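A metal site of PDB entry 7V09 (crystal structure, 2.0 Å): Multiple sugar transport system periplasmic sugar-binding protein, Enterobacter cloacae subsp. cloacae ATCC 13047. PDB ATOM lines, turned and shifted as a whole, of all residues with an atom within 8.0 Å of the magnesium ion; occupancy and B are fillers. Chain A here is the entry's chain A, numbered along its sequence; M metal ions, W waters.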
ATOM      1  N   VAL A 129     -28.107  14.517 -20.014  1.00  0.00           N
ATOM      2  CA  VAL A 129     -29.448  14.644 -19.471  1.00  0.00           C
ATOM      3  C   VAL A 129     -29.473  15.858 -18.542  1.00  0.00           C
ATOM      4  O   VAL A 129     -28.901  15.824 -17.449  1.00  0.00           O
ATOM      5  CB  VAL A 129     -29.883  13.371 -18.744  1.00  0.00           C
ATOM      6  CG1 VAL A 129     -31.372  13.427 -18.444  1.00  0.00           C
ATOM      7  CG2 VAL A 129     -29.541  12.142 -19.558  1.00  0.00           C
ATOM      8  N   TYR A 131     -31.751  18.729 -16.292  1.00  0.00           N
ATOM      9  CA  TYR A 131     -32.951  18.668 -15.473  1.00  0.00           C
ATOM     10  C   TYR A 131     -33.119  19.977 -14.710  1.00  0.00           C
ATOM     11  O   TYR A 131     -32.139  20.682 -14.436  1.00  0.00           O
ATOM     12  CB  TYR A 131     -32.911  17.485 -14.490  1.00  0.00           C
ATOM     13  CG  TYR A 131     -31.896  17.636 -13.377  1.00  0.00           C
ATOM     14  CD1 TYR A 131     -30.577  17.223 -13.554  1.00  0.00           C
ATOM     15  CD2 TYR A 131     -32.258  18.164 -12.137  1.00  0.00           C
ATOM     16  CE1 TYR A 131     -29.651  17.345 -12.531  1.00  0.00           C
ATOM     17  CE2 TYR A 131     -31.331  18.293 -11.126  1.00  0.00           C
ATOM     18  CZ  TYR A 131     -30.031  17.878 -11.315  1.00  0.00           C
ATOM     19  OH  TYR A 131     -29.109  18.008 -10.312  1.00  0.00           O
ATOM     20  N   LYS A 133     -33.567  21.715 -11.350  1.00  0.00           N
ATOM     21  CA  LYS A 133     -33.206  21.327  -9.990  1.00  0.00           C
ATOM     22  C   LYS A 133     -34.399  21.410  -9.048  1.00  0.00           C
ATOM     23  O   LYS A 133     -34.584  20.533  -8.193  1.00  0.00           O
ATOM     24  CB  LYS A 133     -32.063  22.210  -9.477  1.00  0.00           C
ATOM     25  CG  LYS A 133     -30.776  22.095 -10.279  1.00  0.00           C
ATOM     26  CD  LYS A 133     -29.565  22.305  -9.389  1.00  0.00           C
ATOM     27  CE  LYS A 133     -28.600  23.318  -9.979  1.00  0.00           C
ATOM     28  NZ  LYS A 133     -27.376  22.665 -10.522  1.00  0.00           N
ATOM     29  N   GLU A 143     -30.175  13.245  -7.694  1.00  0.00           N
ATOM     30  CA  GLU A 143     -29.550  13.124  -9.002  1.00  0.00           C
ATOM     31  C   GLU A 143     -29.273  11.650  -9.309  1.00  0.00           C
ATOM     32  O   GLU A 143     -28.581  10.992  -8.524  1.00  0.00           O
ATOM     33  CB  GLU A 143     -28.258  13.930  -9.055  1.00  0.00           C
ATOM     34  CG  GLU A 143     -27.401  13.655 -10.287  1.00  0.00           C
ATOM     35  CD  GLU A 143     -26.550  14.844 -10.683  1.00  0.00           C
ATOM     36  OE1 GLU A 143     -26.990  15.995 -10.454  1.00  0.00           O
ATOM     37  OE2 GLU A 143     -25.445  14.631 -11.218  1.00  0.00           O
ATOM     38  N   PRO A 144     -29.810  11.106 -10.399  1.00  0.00           N
ATOM     39  CA  PRO A 144     -29.606   9.673 -10.683  1.00  0.00           C
ATOM     40  C   PRO A 144     -28.129   9.336 -10.825  1.00  0.00           C
ATOM     41  O   PRO A 144     -27.336  10.116 -11.369  1.00  0.00           O
ATOM     42  CB  PRO A 144     -30.355   9.453 -11.996  1.00  0.00           C
ATOM     43  CG  PRO A 144     -31.140  10.684 -12.263  1.00  0.00           C
ATOM     44  CD  PRO A 144     -30.797  11.744 -11.284  1.00  0.00           C
ATOM     45  N   LEU A 261     -30.415  24.877 -13.554  1.00  0.00           N
ATOM     46  CA  LEU A 261     -30.012  23.858 -14.513  1.00  0.00           C
ATOM     47  C   LEU A 261     -29.074  22.852 -13.850  1.00  0.00           C
ATOM     48  O   LEU A 261     -28.043  23.245 -13.282  1.00  0.00           O
ATOM     49  CB  LEU A 261     -29.343  24.493 -15.723  1.00  0.00           C
ATOM     50  CG  LEU A 261     -29.218  23.573 -16.948  1.00  0.00           C
ATOM     51  CD1 LEU A 261     -30.565  22.992 -17.329  1.00  0.00           C
ATOM     52  CD2 LEU A 261     -28.598  24.316 -18.127  1.00  0.00           C
ATOM     53  N   GLY A 262     -29.431  21.571 -13.927  1.00  0.00           N
ATOM     54  CA  GLY A 262     -28.584  20.500 -13.448  1.00  0.00           C
ATOM     55  C   GLY A 262     -28.169  19.579 -14.587  1.00  0.00           C
ATOM     56  O   GLY A 262     -28.702  19.655 -15.701  1.00  0.00           O
ATOM     57  N   PHE A 263     -27.211  18.713 -14.291  1.00  0.00           N
ATOM     58  CA  PHE A 263     -26.644  17.827 -15.296  1.00  0.00           C
ATOM     59  C   PHE A 263     -26.360  16.470 -14.679  1.00  0.00           C
ATOM     60  O   PHE A 263     -25.732  16.378 -13.613  1.00  0.00           O
ATOM     61  CB  PHE A 263     -25.360  18.415 -15.889  1.00  0.00           C
ATOM     62  CG  PHE A 263     -24.834  17.655 -17.079  1.00  0.00           C
ATOM     63  CD1 PHE A 263     -25.436  17.784 -18.309  1.00  0.00           C
ATOM     64  CD2 PHE A 263     -23.731  16.824 -16.961  1.00  0.00           C
ATOM     65  CE1 PHE A 263     -24.962  17.090 -19.411  1.00  0.00           C
ATOM     66  CE2 PHE A 263     -23.245  16.126 -18.047  1.00  0.00           C
ATOM     67  CZ  PHE A 263     -23.863  16.260 -19.276  1.00  0.00           C
ATOM     68  N   VAL A 264     -26.828  15.406 -15.339  1.00  0.00           N
ATOM     69  CA  VAL A 264     -26.495  14.044 -14.949  1.00  0.00           C
ATOM     70  C   VAL A 264     -25.889  13.344 -16.162  1.00  0.00           C
ATOM     71  O   VAL A 264     -26.204  13.670 -17.316  1.00  0.00           O
ATOM     72  CB  VAL A 264     -27.719  13.258 -14.412  1.00  0.00           C
ATOM     73  CG1 VAL A 264     -28.668  14.183 -13.670  1.00  0.00           C
ATOM     74  CG2 VAL A 264     -28.449  12.522 -15.533  1.00  0.00           C
ATOM     75  N   VAL A 265     -24.999  12.400 -15.893  1.00  0.00           N
ATOM     76  CA  VAL A 265     -24.301  11.641 -16.935  1.00  0.00           C
ATOM     77  C   VAL A 265     -24.880  10.227 -16.947  1.00  0.00           C
ATOM     78  O   VAL A 265     -24.869   9.548 -15.910  1.00  0.00           O
ATOM     79  CB  VAL A 265     -22.789  11.610 -16.679  1.00  0.00           C
ATOM     80  CG1 VAL A 265     -22.094  10.771 -17.758  1.00  0.00           C
ATOM     81  CG2 VAL A 265     -22.227  13.021 -16.654  1.00  0.00           C
ATOM     82  N   LEU A 343     -21.595  24.741 -12.820  1.00  0.00           N
ATOM     83  CA  LEU A 343     -21.978  23.844 -13.915  1.00  0.00           C
ATOM     84  C   LEU A 343     -20.965  23.835 -15.062  1.00  0.00           C
ATOM     85  O   LEU A 343     -20.640  22.743 -15.548  1.00  0.00           O
ATOM     86  CB  LEU A 343     -23.382  24.196 -14.417  1.00  0.00           C
ATOM     87  CG  LEU A 343     -23.971  23.257 -15.467  1.00  0.00           C
ATOM     88  CD1 LEU A 343     -24.864  22.211 -14.823  1.00  0.00           C
ATOM     89  CD2 LEU A 343     -24.729  24.048 -16.519  1.00  0.00           C
ATOM     90  N   GLU A 346     -18.219  21.613 -13.869  1.00  0.00           N
ATOM     91  CA  GLU A 346     -18.689  20.238 -13.791  1.00  0.00           C
ATOM     92  C   GLU A 346     -18.779  19.622 -15.177  1.00  0.00           C
ATOM     93  O   GLU A 346     -18.484  18.435 -15.368  1.00  0.00           O
ATOM     94  CB  GLU A 346     -20.030  20.176 -13.069  1.00  0.00           C
ATOM     95  CG  GLU A 346     -20.865  18.952 -13.384  1.00  0.00           C
ATOM     96  CD  GLU A 346     -22.232  18.984 -12.726  1.00  0.00           C
ATOM     97  OE1 GLU A 346     -22.638  20.068 -12.245  1.00  0.00           O
ATOM     98  OE2 GLU A 346     -22.903  17.923 -12.679  1.00  0.00           O
ATOM     99  N   LEU A 347     -19.195  20.412 -16.168  1.00  0.00           N
ATOM    100  CA  LEU A 347     -19.206  19.937 -17.548  1.00  0.00           C
ATOM    101  C   LEU A 347     -17.779  19.721 -18.058  1.00  0.00           C
ATOM    102  O   LEU A 347     -17.509  18.722 -18.726  1.00  0.00           O
ATOM    103  CB  LEU A 347     -19.954  20.929 -18.443  1.00  0.00           C
ATOM    104  CG  LEU A 347     -21.456  21.061 -18.208  1.00  0.00           C
ATOM    105  CD1 LEU A 347     -22.018  22.262 -18.950  1.00  0.00           C
ATOM    106  CD2 LEU A 347     -22.170  19.791 -18.635  1.00  0.00           C
ATOM    107  N   GLN A 350     -16.237  16.568 -16.964  1.00  0.00           N
ATOM    108  CA  GLN A 350     -16.746  15.368 -17.607  1.00  0.00           C
ATOM    109  C   GLN A 350     -16.028  15.048 -18.920  1.00  0.00           C
ATOM    110  O   GLN A 350     -16.440  14.115 -19.621  1.00  0.00           O
ATOM    111  CB  GLN A 350     -18.246  15.512 -17.862  1.00  0.00           C
ATOM    112  CG  GLN A 350     -19.115  15.170 -16.662  1.00  0.00           C
ATOM    113  CD  GLN A 350     -18.651  13.913 -15.945  1.00  0.00           C
ATOM    114  OE1 GLN A 350     -18.545  12.847 -16.554  1.00  0.00           O
ATOM    115  NE2 GLN A 350     -18.371  14.035 -14.656  1.00  0.00           N
HETATM  116 MG    MG M   1     -24.738  16.843 -11.794  1.00  0.00          MG
HETATM  117  O   HOH W   1     -23.309  16.553 -10.013  1.00  0.00           O
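The side-chain hydroxyl (OH) of Tyr 131 lies within hydrogen-bond range of the side-chain carboxylate (OE1) of Glu 143 (2.9 Å).
Three residues have an atom within 4 Å of the magnesium ion: Glu 143, Phe 263 and Glu 346.
Along chain A the residues within 4 Å of the magnesium ion span positions 143 to 346.
The magnesium ion is bound by O of Phe 263 (2.1 Å), water W1 (2.3 Å), OE2 of Glu 346 (2.3 Å) and OE2 of Glu 143 (2.4 Å).
The magnesium ion has four donor atoms within binding distance.
Slightly farther from the magnesium ion lies OE1 of Glu 143 (2.8 Å).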
